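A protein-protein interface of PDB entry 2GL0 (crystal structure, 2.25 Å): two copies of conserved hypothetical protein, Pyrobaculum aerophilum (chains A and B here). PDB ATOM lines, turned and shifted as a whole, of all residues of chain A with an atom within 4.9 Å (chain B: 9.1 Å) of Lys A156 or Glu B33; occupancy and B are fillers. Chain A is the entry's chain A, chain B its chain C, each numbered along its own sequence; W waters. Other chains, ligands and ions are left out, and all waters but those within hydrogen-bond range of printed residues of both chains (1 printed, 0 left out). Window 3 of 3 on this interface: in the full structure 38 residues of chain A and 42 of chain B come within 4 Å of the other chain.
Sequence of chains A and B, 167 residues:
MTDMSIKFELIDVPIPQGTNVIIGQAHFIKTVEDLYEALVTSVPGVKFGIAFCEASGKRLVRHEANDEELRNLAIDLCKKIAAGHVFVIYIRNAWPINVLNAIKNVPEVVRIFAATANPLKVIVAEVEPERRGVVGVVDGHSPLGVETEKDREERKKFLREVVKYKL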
ATOM      1  N   ARG A 152       1.998  15.918  22.558  1.00  0.00           N
ATOM      2  CA  ARG A 152       1.184  16.779  21.655  1.00  0.00           C
ATOM      3  C   ARG A 152      -0.021  16.007  21.079  1.00  0.00           C
ATOM      4  O   ARG A 152      -1.170  16.554  21.039  1.00  0.00           O
ATOM      5  CB  ARG A 152       2.029  17.346  20.541  1.00  0.00           C
ATOM      6  CG  ARG A 152       1.245  17.923  19.390  1.00  0.00           C
ATOM      7  CD  ARG A 152       2.135  18.676  18.379  1.00  0.00           C
ATOM      8  NE  ARG A 152       1.345  19.468  17.419  1.00  0.00           N
ATOM      9  CZ  ARG A 152       0.776  18.989  16.291  1.00  0.00           C
ATOM     10  NH1 ARG A 152       0.873  17.703  15.938  1.00  0.00           N
ATOM     11  NH2 ARG A 152       0.074  19.801  15.510  1.00  0.00           N
ATOM     12  N   GLU A 153       0.235  14.756  20.632  1.00  0.00           N
ATOM     13  CA  GLU A 153      -0.817  13.789  20.211  1.00  0.00           C
ATOM     14  C   GLU A 153      -1.900  13.557  21.279  1.00  0.00           C
ATOM     15  O   GLU A 153      -3.123  13.533  20.990  1.00  0.00           O
ATOM     16  CB  GLU A 153      -0.221  12.428  19.833  1.00  0.00           C
ATOM     17  CG  GLU A 153       0.477  12.380  18.472  1.00  0.00           C
ATOM     18  CD  GLU A 153      -0.188  13.274  17.389  1.00  0.00           C
ATOM     19  OE1 GLU A 153      -1.463  13.342  17.289  1.00  0.00           O
ATOM     20  OE2 GLU A 153       0.590  13.894  16.624  1.00  0.00           O
ATOM     21  N   GLU A 154      -1.429  13.400  22.512  1.00  0.00           N
ATOM     22  CA  GLU A 154      -2.294  13.217  23.654  1.00  0.00           C
ATOM     23  C   GLU A 154      -3.064  14.526  23.907  1.00  0.00           C
ATOM     24  O   GLU A 154      -4.290  14.501  24.064  1.00  0.00           O
ATOM     25  CB  GLU A 154      -1.472  12.707  24.861  1.00  0.00           C
ATOM     26  CG  GLU A 154      -0.939  11.239  24.613  1.00  0.00           C
ATOM     27  CD  GLU A 154       0.081  10.769  25.684  1.00  0.00           C
ATOM     28  OE1 GLU A 154       0.062  11.391  26.813  1.00  0.00           O
ATOM     29  OE2 GLU A 154       0.883   9.810  25.387  1.00  0.00           O
ATOM     30  N   ARG A 155      -2.364  15.665  23.891  1.00  0.00           N
ATOM     31  CA  ARG A 155      -3.031  16.960  24.022  1.00  0.00           C
ATOM     32  C   ARG A 155      -4.109  17.191  22.913  1.00  0.00           C
ATOM     33  O   ARG A 155      -5.267  17.601  23.241  1.00  0.00           O
ATOM     34  CB  ARG A 155      -2.003  18.104  24.103  1.00  0.00           C
ATOM     35  CG  ARG A 155      -2.574  19.481  23.930  1.00  0.00           C
ATOM     36  CD  ARG A 155      -1.493  20.406  23.319  1.00  0.00           C
ATOM     37  NE  ARG A 155      -1.713  20.675  21.906  1.00  0.00           N
ATOM     38  CZ  ARG A 155      -0.773  21.083  21.052  1.00  0.00           C
ATOM     39  NH1 ARG A 155       0.520  21.274  21.387  1.00  0.00           N
ATOM     40  NH2 ARG A 155      -1.154  21.300  19.812  1.00  0.00           N
ATOM     41  N   LYS A 156      -3.758  16.907  21.644  1.00  0.00           N
ATOM     42  CA  LYS A 156      -4.682  17.081  20.529  1.00  0.00           C
ATOM     43  C   LYS A 156      -5.881  16.168  20.692  1.00  0.00           C
ATOM     44  O   LYS A 156      -6.977  16.550  20.361  1.00  0.00           O
ATOM     45  CB  LYS A 156      -4.017  16.777  19.183  1.00  0.00           C
ATOM     46  CG  LYS A 156      -3.177  17.875  18.583  1.00  0.00           C
ATOM     47  CD  LYS A 156      -2.157  17.288  17.647  1.00  0.00           C
ATOM     48  CE  LYS A 156      -2.686  16.994  16.233  1.00  0.00           C
ATOM     49  NZ  LYS A 156      -2.180  15.589  15.801  1.00  0.00           N
ATOM     50  N   LYS A 157      -5.684  14.962  21.217  1.00  0.00           N
ATOM     51  CA  LYS A 157      -6.814  14.050  21.478  1.00  0.00           C
ATOM     52  C   LYS A 157      -7.611  14.469  22.704  1.00  0.00           C
ATOM     53  O   LYS A 157      -8.790  14.243  22.754  1.00  0.00           O
ATOM     54  CB  LYS A 157      -6.333  12.587  21.618  1.00  0.00           C
ATOM     55  CG  LYS A 157      -5.772  11.996  20.318  1.00  0.00           C
ATOM     56  CD  LYS A 157      -5.266  10.525  20.438  1.00  0.00           C
ATOM     57  CE  LYS A 157      -6.273   9.589  21.123  1.00  0.00           C
ATOM     58  NZ  LYS A 157      -5.619   8.593  22.055  1.00  0.00           N
ATOM     59  N   PHE A 158      -6.980  15.071  23.706  1.00  0.00           N
ATOM     60  CA  PHE A 158      -7.741  15.591  24.847  1.00  0.00           C
ATOM     61  C   PHE A 158      -8.781  16.626  24.378  1.00  0.00           C
ATOM     62  O   PHE A 158      -9.932  16.500  24.734  1.00  0.00           O
ATOM     63  CB  PHE A 158      -6.814  16.086  25.966  1.00  0.00           C
ATOM     64  CG  PHE A 158      -7.451  17.053  26.872  1.00  0.00           C
ATOM     65  CD1 PHE A 158      -8.326  16.632  27.872  1.00  0.00           C
ATOM     66  CD2 PHE A 158      -7.188  18.418  26.744  1.00  0.00           C
ATOM     67  CE1 PHE A 158      -8.966  17.567  28.706  1.00  0.00           C
ATOM     68  CE2 PHE A 158      -7.798  19.329  27.579  1.00  0.00           C
ATOM     69  CZ  PHE A 158      -8.711  18.919  28.537  1.00  0.00           C
ATOM     70  N   LEU A 159      -8.371  17.594  23.527  1.00  0.00           N
ATOM     71  CA  LEU A 159      -9.239  18.695  23.021  1.00  0.00           C
ATOM     72  C   LEU A 159     -10.372  18.224  22.091  1.00  0.00           C
ATOM     73  O   LEU A 159     -11.482  18.756  22.121  1.00  0.00           O
ATOM     74  CB  LEU A 159      -8.394  19.728  22.325  1.00  0.00           C
ATOM     75  CG  LEU A 159      -7.454  20.498  23.292  1.00  0.00           C
ATOM     76  CD1 LEU A 159      -6.717  21.444  22.488  1.00  0.00           C
ATOM     77  CD2 LEU A 159      -8.234  21.231  24.349  1.00  0.00           C
ATOM     78  N   ARG A 160     -10.097  17.148  21.350  1.00  0.00           N
ATOM     79  CA  ARG A 160     -10.990  16.668  20.335  1.00  0.00           C
ATOM     80  C   ARG A 160     -11.899  15.499  20.804  1.00  0.00           C
ATOM     81  O   ARG A 160     -13.018  15.385  20.352  1.00  0.00           O
ATOM     82  CB  ARG A 160     -10.178  16.214  19.115  1.00  0.00           C
ATOM     83  CG  ARG A 160      -9.724  17.313  18.322  1.00  0.00           C
ATOM     84  CD  ARG A 160      -8.610  16.887  17.480  1.00  0.00           C
ATOM     85  NE  ARG A 160      -8.060  18.063  16.846  1.00  0.00           N
ATOM     86  CZ  ARG A 160      -7.355  19.000  17.495  1.00  0.00           C
ATOM     87  NH1 ARG A 160      -7.114  18.833  18.785  1.00  0.00           N
ATOM     88  NH2 ARG A 160      -6.873  20.077  16.867  1.00  0.00           N
ATOM     89  N   LYS A 166     -12.254  21.138  19.860  1.00  0.00           N
ATOM     90  CA  LYS A 166     -11.566  21.091  18.561  1.00  0.00           C
ATOM     91  C   LYS A 166     -12.094  19.909  17.736  1.00  0.00           C
ATOM     92  O   LYS A 166     -12.722  19.015  18.295  1.00  0.00           O
ATOM     93  CB  LYS A 166     -10.026  21.027  18.735  1.00  0.00           C
ATOM     94  CG  LYS A 166      -9.374  22.326  19.346  1.00  0.00           C
ATOM     95  CD  LYS A 166      -9.473  23.598  18.436  1.00  0.00           C
ATOM     96  CE  LYS A 166      -8.823  24.818  19.047  1.00  0.00           C
ATOM     97  NZ  LYS A 166      -9.132  26.005  18.195  1.00  0.00           N
ATOM     98  N   PHE B  28      -5.452  27.677  30.291  1.00  0.00           N
ATOM     99  CA  PHE B  28      -6.041  26.492  29.676  1.00  0.00           C
ATOM    100  C   PHE B  28      -5.254  26.094  28.448  1.00  0.00           C
ATOM    101  O   PHE B  28      -4.942  26.948  27.569  1.00  0.00           O
ATOM    102  CB  PHE B  28      -7.525  26.739  29.333  1.00  0.00           C
ATOM    103  CG  PHE B  28      -8.251  25.525  28.773  1.00  0.00           C
ATOM    104  CD1 PHE B  28      -8.004  24.231  29.284  1.00  0.00           C
ATOM    105  CD2 PHE B  28      -9.161  25.677  27.723  1.00  0.00           C
ATOM    106  CE1 PHE B  28      -8.621  23.127  28.727  1.00  0.00           C
ATOM    107  CE2 PHE B  28      -9.789  24.547  27.177  1.00  0.00           C
ATOM    108  CZ  PHE B  28      -9.524  23.294  27.689  1.00  0.00           C
ATOM    109  N   ILE B  29      -5.014  24.788  28.352  1.00  0.00           N
ATOM    110  CA  ILE B  29      -4.249  24.099  27.302  1.00  0.00           C
ATOM    111  C   ILE B  29      -4.637  24.489  25.850  1.00  0.00           C
ATOM    112  O   ILE B  29      -3.811  24.479  24.936  1.00  0.00           O
ATOM    113  CB  ILE B  29      -4.262  22.482  27.580  1.00  0.00           C
ATOM    114  CG1 ILE B  29      -3.026  21.770  26.963  1.00  0.00           C
ATOM    115  CG2 ILE B  29      -5.553  21.761  27.150  1.00  0.00           C
ATOM    116  CD1 ILE B  29      -1.778  22.198  27.646  1.00  0.00           C
ATOM    117  N   LYS B  30      -5.906  24.858  25.684  1.00  0.00           N
ATOM    118  CA  LYS B  30      -6.491  25.147  24.405  1.00  0.00           C
ATOM    119  C   LYS B  30      -5.812  26.431  23.845  1.00  0.00           C
ATOM    120  O   LYS B  30      -5.676  26.612  22.611  1.00  0.00           O
ATOM    121  CB  LYS B  30      -8.070  25.170  24.489  1.00  0.00           C
ATOM    122  CG  LYS B  30      -8.697  25.133  23.079  1.00  0.00           C
ATOM    123  CD  LYS B  30     -10.153  24.862  23.000  1.00  0.00           C
ATOM    124  CE  LYS B  30     -10.995  26.004  23.559  1.00  0.00           C
ATOM    125  NZ  LYS B  30     -11.303  27.103  22.586  1.00  0.00           N
ATOM    126  N   THR B  31      -5.247  27.255  24.755  1.00  0.00           N
ATOM    127  CA  THR B  31      -4.437  28.426  24.370  1.00  0.00           C
ATOM    128  C   THR B  31      -3.533  28.214  23.153  1.00  0.00           C
ATOM    129  O   THR B  31      -3.518  29.041  22.223  1.00  0.00           O
ATOM    130  CB  THR B  31      -3.630  28.893  25.575  1.00  0.00           C
ATOM    131  OG1 THR B  31      -4.562  29.311  26.617  1.00  0.00           O
ATOM    132  CG2 THR B  31      -2.519  29.994  25.193  1.00  0.00           C
ATOM    133  N   VAL B  32      -2.756  27.131  23.148  1.00  0.00           N
ATOM    134  CA  VAL B  32      -1.744  26.879  22.124  1.00  0.00           C
ATOM    135  C   VAL B  32      -2.290  26.673  20.673  1.00  0.00           C
ATOM    136  O   VAL B  32      -1.648  27.139  19.689  1.00  0.00           O
ATOM    137  CB  VAL B  32      -0.769  25.693  22.588  1.00  0.00           C
ATOM    138  CG1 VAL B  32      -1.306  24.338  22.223  1.00  0.00           C
ATOM    139  CG2 VAL B  32       0.568  25.880  22.034  1.00  0.00           C
ATOM    140  N   GLU B  33      -3.457  26.014  20.550  1.00  0.00           N
ATOM    141  CA  GLU B  33      -4.096  25.803  19.247  1.00  0.00           C
ATOM    142  C   GLU B  33      -4.747  27.068  18.816  1.00  0.00           C
ATOM    143  O   GLU B  33      -4.611  27.421  17.666  1.00  0.00           O
ATOM    144  CB  GLU B  33      -5.130  24.654  19.243  1.00  0.00           C
ATOM    145  CG  GLU B  33      -4.552  23.260  19.669  1.00  0.00           C
ATOM    146  CD  GLU B  33      -5.283  22.014  19.069  1.00  0.00           C
ATOM    147  OE1 GLU B  33      -6.182  22.122  18.182  1.00  0.00           O
ATOM    148  OE2 GLU B  33      -4.935  20.883  19.499  1.00  0.00           O
ATOM    149  N   ASP B  34      -5.427  27.744  19.743  1.00  0.00           N
ATOM    150  CA  ASP B  34      -6.119  29.026  19.500  1.00  0.00           C
ATOM    151  C   ASP B  34      -5.225  30.168  19.085  1.00  0.00           C
ATOM    152  O   ASP B  34      -5.591  30.883  18.162  1.00  0.00           O
ATOM    153  CB  ASP B  34      -6.996  29.477  20.703  1.00  0.00           C
ATOM    154  CG  ASP B  34      -8.248  28.683  20.855  1.00  0.00           C
ATOM    155  OD1 ASP B  34      -8.616  27.832  20.007  1.00  0.00           O
ATOM    156  OD2 ASP B  34      -8.914  28.926  21.872  1.00  0.00           O
ATOM    157  N   LEU B  35      -4.078  30.332  19.752  1.00  0.00           N
ATOM    158  CA  LEU B  35      -3.012  31.201  19.270  1.00  0.00           C
ATOM    159  C   LEU B  35      -2.443  30.850  17.874  1.00  0.00           C
ATOM    160  O   LEU B  35      -2.189  31.747  17.069  1.00  0.00           O
ATOM    161  CB  LEU B  35      -1.907  31.386  20.319  1.00  0.00           C
ATOM    162  CG  LEU B  35      -2.315  32.183  21.593  1.00  0.00           C
ATOM    163  CD1 LEU B  35      -1.214  32.299  22.546  1.00  0.00           C
ATOM    164  CD2 LEU B  35      -2.823  33.598  21.329  1.00  0.00           C
ATOM    165  N   TYR B  36      -2.292  29.552  17.564  1.00  0.00           N
ATOM    166  CA  TYR B  36      -1.754  29.101  16.274  1.00  0.00           C
ATOM    167  C   TYR B  36      -2.736  29.506  15.158  1.00  0.00           C
ATOM    168  O   TYR B  36      -2.323  30.097  14.131  1.00  0.00           O
ATOM    169  CB  TYR B  36      -1.496  27.584  16.262  1.00  0.00           C
ATOM    170  CG  TYR B  36      -1.345  26.993  14.852  1.00  0.00           C
ATOM    171  CD1 TYR B  36      -2.454  26.692  14.041  1.00  0.00           C
ATOM    172  CD2 TYR B  36      -0.093  26.763  14.343  1.00  0.00           C
ATOM    173  CE1 TYR B  36      -2.276  26.197  12.731  1.00  0.00           C
ATOM    174  CE2 TYR B  36       0.111  26.247  13.025  1.00  0.00           C
ATOM    175  CZ  TYR B  36      -0.963  25.973  12.223  1.00  0.00           C
ATOM    176  OH  TYR B  36      -0.669  25.472  10.937  1.00  0.00           O
ATOM    177  N   GLU B  37      -4.030  29.217  15.358  1.00  0.00           N
ATOM    178  CA  GLU B  37      -5.081  29.650  14.423  1.00  0.00           C
ATOM    179  C   GLU B  37      -5.230  31.205  14.230  1.00  0.00           C
ATOM    180  O   GLU B  37      -5.429  31.657  13.093  1.00  0.00           O
ATOM    181  CB  GLU B  37      -6.405  29.026  14.840  1.00  0.00           C
ATOM    182  CG  GLU B  37      -6.423  27.418  14.957  1.00  0.00           C
ATOM    183  CD  GLU B  37      -7.821  26.928  15.183  1.00  0.00           C
ATOM    184  OE1 GLU B  37      -8.786  27.655  14.822  1.00  0.00           O
ATOM    185  OE2 GLU B  37      -7.998  25.838  15.743  1.00  0.00           O
ATOM    186  N   ALA B  38      -5.121  31.991  15.324  1.00  0.00           N
ATOM    187  CA  ALA B  38      -5.120  33.463  15.287  1.00  0.00           C
ATOM    188  C   ALA B  38      -4.022  33.927  14.358  1.00  0.00           C
ATOM    189  O   ALA B  38      -4.269  34.784  13.514  1.00  0.00           O
ATOM    190  CB  ALA B  38      -4.917  34.050  16.682  1.00  0.00           C
ATOM    191  N   LEU B  39      -2.823  33.336  14.485  1.00  0.00           N
ATOM    192  CA  LEU B  39      -1.675  33.705  13.669  1.00  0.00           C
ATOM    193  C   LEU B  39      -1.823  33.293  12.225  1.00  0.00           C
ATOM    194  O   LEU B  39      -1.711  34.124  11.329  1.00  0.00           O
ATOM    195  CB  LEU B  39      -0.332  33.240  14.305  1.00  0.00           C
ATOM    196  CG  LEU B  39       0.180  33.835  15.617  1.00  0.00           C
ATOM    197  CD1 LEU B  39       1.167  32.983  16.359  1.00  0.00           C
ATOM    198  CD2 LEU B  39       0.869  35.136  15.383  1.00  0.00           C
ATOM    199  N   VAL B  40      -2.129  32.041  11.959  1.00  0.00           N
ATOM    200  CA  VAL B  40      -2.148  31.572  10.556  1.00  0.00           C
ATOM    201  C   VAL B  40      -3.325  32.117   9.690  1.00  0.00           C
ATOM    202  O   VAL B  40      -3.289  32.096   8.440  1.00  0.00           O
ATOM    203  CB  VAL B  40      -1.978  30.001  10.511  1.00  0.00           C
ATOM    204  CG1 VAL B  40      -3.273  29.214  11.119  1.00  0.00           C
ATOM    205  CG2 VAL B  40      -1.517  29.485   9.071  1.00  0.00           C
ATOM    206  N   THR B  41      -4.367  32.613  10.344  1.00  0.00           N
ATOM    207  CA  THR B  41      -5.532  33.160   9.652  1.00  0.00           C
ATOM    208  C   THR B  41      -5.513  34.730   9.591  1.00  0.00           C
ATOM    209  O   THR B  41      -6.415  35.392   9.047  1.00  0.00           O
ATOM    210  CB  THR B  41      -6.811  32.574  10.212  1.00  0.00           C
ATOM    211  OG1 THR B  41      -6.987  32.995  11.570  1.00  0.00           O
ATOM    212  CG2 THR B  41      -6.789  31.062  10.177  1.00  0.00           C
ATOM    213  N   PHE B  48       5.909  31.774  12.220  1.00  0.00           N
ATOM    214  CA  PHE B  48       5.848  32.031  13.661  1.00  0.00           C
ATOM    215  C   PHE B  48       6.159  30.787  14.438  1.00  0.00           C
ATOM    216  O   PHE B  48       6.075  29.694  13.937  1.00  0.00           O
ATOM    217  CB  PHE B  48       4.439  32.473  14.087  1.00  0.00           C
ATOM    218  CG  PHE B  48       3.408  31.447  13.790  1.00  0.00           C
ATOM    219  CD1 PHE B  48       3.059  30.491  14.724  1.00  0.00           C
ATOM    220  CD2 PHE B  48       2.833  31.374  12.527  1.00  0.00           C
ATOM    221  CE1 PHE B  48       2.128  29.499  14.418  1.00  0.00           C
ATOM    222  CE2 PHE B  48       1.878  30.393  12.224  1.00  0.00           C
ATOM    223  CZ  PHE B  48       1.527  29.481  13.184  1.00  0.00           C
ATOM    224  N   ILE B  50       4.969  29.614  18.500  1.00  0.00           N
ATOM    225  CA  ILE B  50       4.177  29.926  19.666  1.00  0.00           C
ATOM    226  C   ILE B  50       4.406  28.852  20.778  1.00  0.00           C
ATOM    227  O   ILE B  50       4.463  27.668  20.505  1.00  0.00           O
ATOM    228  CB  ILE B  50       2.612  30.184  19.350  1.00  0.00           C
ATOM    229  CG1 ILE B  50       1.774  29.791  20.539  1.00  0.00           C
ATOM    230  CG2 ILE B  50       2.040  29.426  18.197  1.00  0.00           C
ATOM    231  CD1 ILE B  50       1.880  30.725  21.553  1.00  0.00           C
ATOM    232  N   ALA B  51       4.556  29.282  22.025  1.00  0.00           N
ATOM    233  CA  ALA B  51       4.770  28.363  23.132  1.00  0.00           C
ATOM    234  C   ALA B  51       3.930  28.793  24.364  1.00  0.00           C
ATOM    235  O   ALA B  51       3.698  29.986  24.586  1.00  0.00           O
ATOM    236  CB  ALA B  51       6.262  28.261  23.457  1.00  0.00           C
ATOM    237  N   PHE B  52       3.436  27.837  25.134  1.00  0.00           N
ATOM    238  CA  PHE B  52       2.602  28.161  26.238  1.00  0.00           C
ATOM    239  C   PHE B  52       3.100  27.373  27.437  1.00  0.00           C
ATOM    240  O   PHE B  52       3.492  26.216  27.309  1.00  0.00           O
ATOM    241  CB  PHE B  52       1.143  27.861  25.838  1.00  0.00           C
ATOM    242  CG  PHE B  52       0.124  27.884  26.973  1.00  0.00           C
ATOM    243  CD1 PHE B  52      -0.259  29.112  27.589  1.00  0.00           C
ATOM    244  CD2 PHE B  52      -0.563  26.709  27.337  1.00  0.00           C
ATOM    245  CE1 PHE B  52      -1.181  29.151  28.570  1.00  0.00           C
ATOM    246  CE2 PHE B  52      -1.516  26.784  28.326  1.00  0.00           C
ATOM    247  CZ  PHE B  52      -1.813  28.015  28.950  1.00  0.00           C
ATOM    248  N   ARG B  62       4.058  23.780  25.814  1.00  0.00           N
ATOM    249  CA  ARG B  62       3.337  23.360  24.576  1.00  0.00           C
ATOM    250  C   ARG B  62       3.670  24.370  23.498  1.00  0.00           C
ATOM    251  O   ARG B  62       3.671  25.605  23.774  1.00  0.00           O
ATOM    252  CB  ARG B  62       1.806  23.334  24.739  1.00  0.00           C
ATOM    253  CG  ARG B  62       1.270  22.743  26.069  1.00  0.00           C
ATOM    254  CD  ARG B  62       1.577  21.232  26.112  1.00  0.00           C
ATOM    255  NE  ARG B  62       1.241  20.554  27.369  1.00  0.00           N
ATOM    256  CZ  ARG B  62       0.900  19.279  27.437  1.00  0.00           C
ATOM    257  NH1 ARG B  62       0.851  18.555  26.343  1.00  0.00           N
ATOM    258  NH2 ARG B  62       0.607  18.734  28.574  1.00  0.00           N
ATOM    259  N   HIS B  63       3.970  23.872  22.283  1.00  0.00           N
ATOM    260  CA  HIS B  63       4.322  24.725  21.118  1.00  0.00           C
ATOM    261  C   HIS B  63       3.699  24.266  19.755  1.00  0.00           C
ATOM    262  O   HIS B  63       3.296  23.115  19.583  1.00  0.00           O
ATOM    263  CB  HIS B  63       5.847  24.756  21.013  1.00  0.00           C
ATOM    264  CG  HIS B  63       6.472  23.393  21.183  1.00  0.00           C
ATOM    265  ND1 HIS B  63       6.987  22.668  20.127  1.00  0.00           N
ATOM    266  CD2 HIS B  63       6.639  22.623  22.288  1.00  0.00           C
ATOM    267  CE1 HIS B  63       7.444  21.515  20.583  1.00  0.00           C
ATOM    268  NE2 HIS B  63       7.247  21.464  21.887  1.00  0.00           N
ATOM    269  N   GLU B  64       3.602  25.203  18.825  1.00  0.00           N
ATOM    270  CA  GLU B  64       3.138  24.998  17.466  1.00  0.00           C
ATOM    271  C   GLU B  64       3.962  26.006  16.738  1.00  0.00           C
ATOM    272  O   GLU B  64       4.279  27.108  17.285  1.00  0.00           O
ATOM    273  CB  GLU B  64       1.657  25.394  17.270  1.00  0.00           C
ATOM    274  CG  GLU B  64       0.604  24.428  17.845  1.00  0.00           C
ATOM    275  CD  GLU B  64       0.722  22.961  17.352  1.00  0.00           C
ATOM    276  OE1 GLU B  64       1.495  22.638  16.364  1.00  0.00           O
ATOM    277  OE2 GLU B  64       0.012  22.114  17.952  1.00  0.00           O
ATOM    278  N   VAL B 106      -8.866  36.098  21.781  1.00  0.00           N
ATOM    279  CA  VAL B 106      -8.812  34.658  21.952  1.00  0.00           C
ATOM    280  C   VAL B 106      -9.331  34.519  23.347  1.00  0.00           C
ATOM    281  O   VAL B 106      -8.759  35.112  24.214  1.00  0.00           O
ATOM    282  CB  VAL B 106      -7.331  34.123  21.718  1.00  0.00           C
ATOM    283  CG1 VAL B 106      -7.102  32.824  22.428  1.00  0.00           C
ATOM    284  CG2 VAL B 106      -7.117  33.863  20.219  1.00  0.00           C
ATOM    285  N   GLU B 108      -8.951  32.497  25.776  1.00  0.00           N
ATOM    286  CA  GLU B 108      -8.078  32.022  26.820  1.00  0.00           C
ATOM    287  C   GLU B 108      -7.139  33.212  27.268  1.00  0.00           C
ATOM    288  O   GLU B 108      -6.708  33.250  28.431  1.00  0.00           O
ATOM    289  CB  GLU B 108      -7.259  30.826  26.338  1.00  0.00           C
ATOM    290  CG  GLU B 108      -7.974  29.402  26.222  1.00  0.00           C
ATOM    291  CD  GLU B 108      -8.691  29.188  24.918  1.00  0.00           C
ATOM    292  OE1 GLU B 108      -8.321  29.808  23.914  1.00  0.00           O
ATOM    293  OE2 GLU B 108      -9.655  28.423  24.857  1.00  0.00           O
HETATM  294  O   HOH W   1       4.205  21.034  16.388  1.00  0.00           O
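The side-chain carboxylate of Glu B64 lies within salt-bridge range of the guanidinium group of Arg A152 (3.0 Å).
NH2 of Arg A155 is in salt-bridge range of OE2 of Glu B33, at 3.8 Å.
The guanidinium group of Arg A155 is in salt-bridge range of the side-chain carboxylate of Glu B64 (3.6 Å).
The side-chain carboxylate (OE1) of Glu B33 is in salt-bridge range of the guanidinium group (NH2) of Arg A160, 2.5 Å away.
The side-chain carboxylate (OD1) of Asp B34 lies within salt-bridge range of the side-chain amino group (NZ) of Lys A166, at 2.6 Å.
The side-chain amino group of Lys A166 lies within salt-bridge range of the side-chain carboxylate of Glu B37, at 2.7 Å.
The side-chain carboxylate of Glu A153 is in salt-bridge range of the guanidinium group of Arg A152, 3.9 Å away.
The guanidinium group (NH1) of Arg A160 sits at hydrogen-bond distance from the backbone carbonyl oxygen (O) of Lys A156 (2.8 Å).
The backbone NH of Lys A166 sits at hydrogen-bond distance from the backbone carbonyl oxygen of Leu A159, 3.4 Å away.
NZ of Lys B30 lies within salt-bridge range of OD2 of Asp B34.
The backbone NH of Ile B50 sits at hydrogen-bond distance from the backbone carbonyl oxygen of Glu B64 (2.9 Å).
N of Phe B52 sits at hydrogen-bond distance from O of Arg B62.
Among the printed residues, merely in contact across the chains: Arg A155 with Ile B29 (3.8 Å), Arg A155 with Val B32 (3.5 Å), Arg A155 with Arg B62 (3.7 Å), Arg A155 with His B63 (3.8 Å), Lys A156 with Glu B33 (3.6 Å), Phe A158 with Ile B29 (3.3 Å), Leu A159 with Ile B29 (3.9 Å), Leu A159 with Lys B30 (3.9 Å), Leu A159 with Glu B33 (3.5 Å) and Lys A166 with Glu B33 (3.4 Å).
Lys A156 touches just one residue of chain B: Glu B33.
Printed residues of chain A within 4 Å of Glu B33: Arg A155, Lys A156, Leu A159, Arg A160 and Lys A166.
Of the printed residues of chain A, Ile B29 touches Arg A155, Phe A158 and Leu A159.
Printed residues of chain A within 4 Å of His B63: Arg A155.
Leu B39 touches none of the printed residues of chain A.
The nearest residue of chain B that does not touch Lys A156 is Glu B64 (5.3 Å).
The nearest printed residue of chain A that does not touch Lys B30 is Lys A166 (4.05 Å).
Along chain B the printed residues that touch a printed residue of chain A span positions 29 to 64.
Printed residues of chain A that touch a printed residue of chain B: Arg A152, Arg A155, Lys A156, Phe A158, Leu A159, Arg A160 and Lys A166.
Hydrophobic or aromatic side chains of chain A within 4 Å of the printed part of chain B: Phe A158 and Leu A159.
Among the printed residues, Asp or Glu carboxylates within 4 Å of a Lys or Arg side-chain nitrogen of the other chain: Arg A152 with Glu B64 (3.0 Å), Arg A155 with Glu B33 (3.8 Å), Arg A155 with Glu B64 (2.3 Å), Arg A160 with Glu B33 (2.5 Å), Lys A166 with Asp B34 (2.6 Å) and Lys A166 with Glu B37 (2.7 Å).
No position is printed for both chains.
Water W1 lies within hydrogen-bond range of OE1 of Glu B64 and NE of Arg A152.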
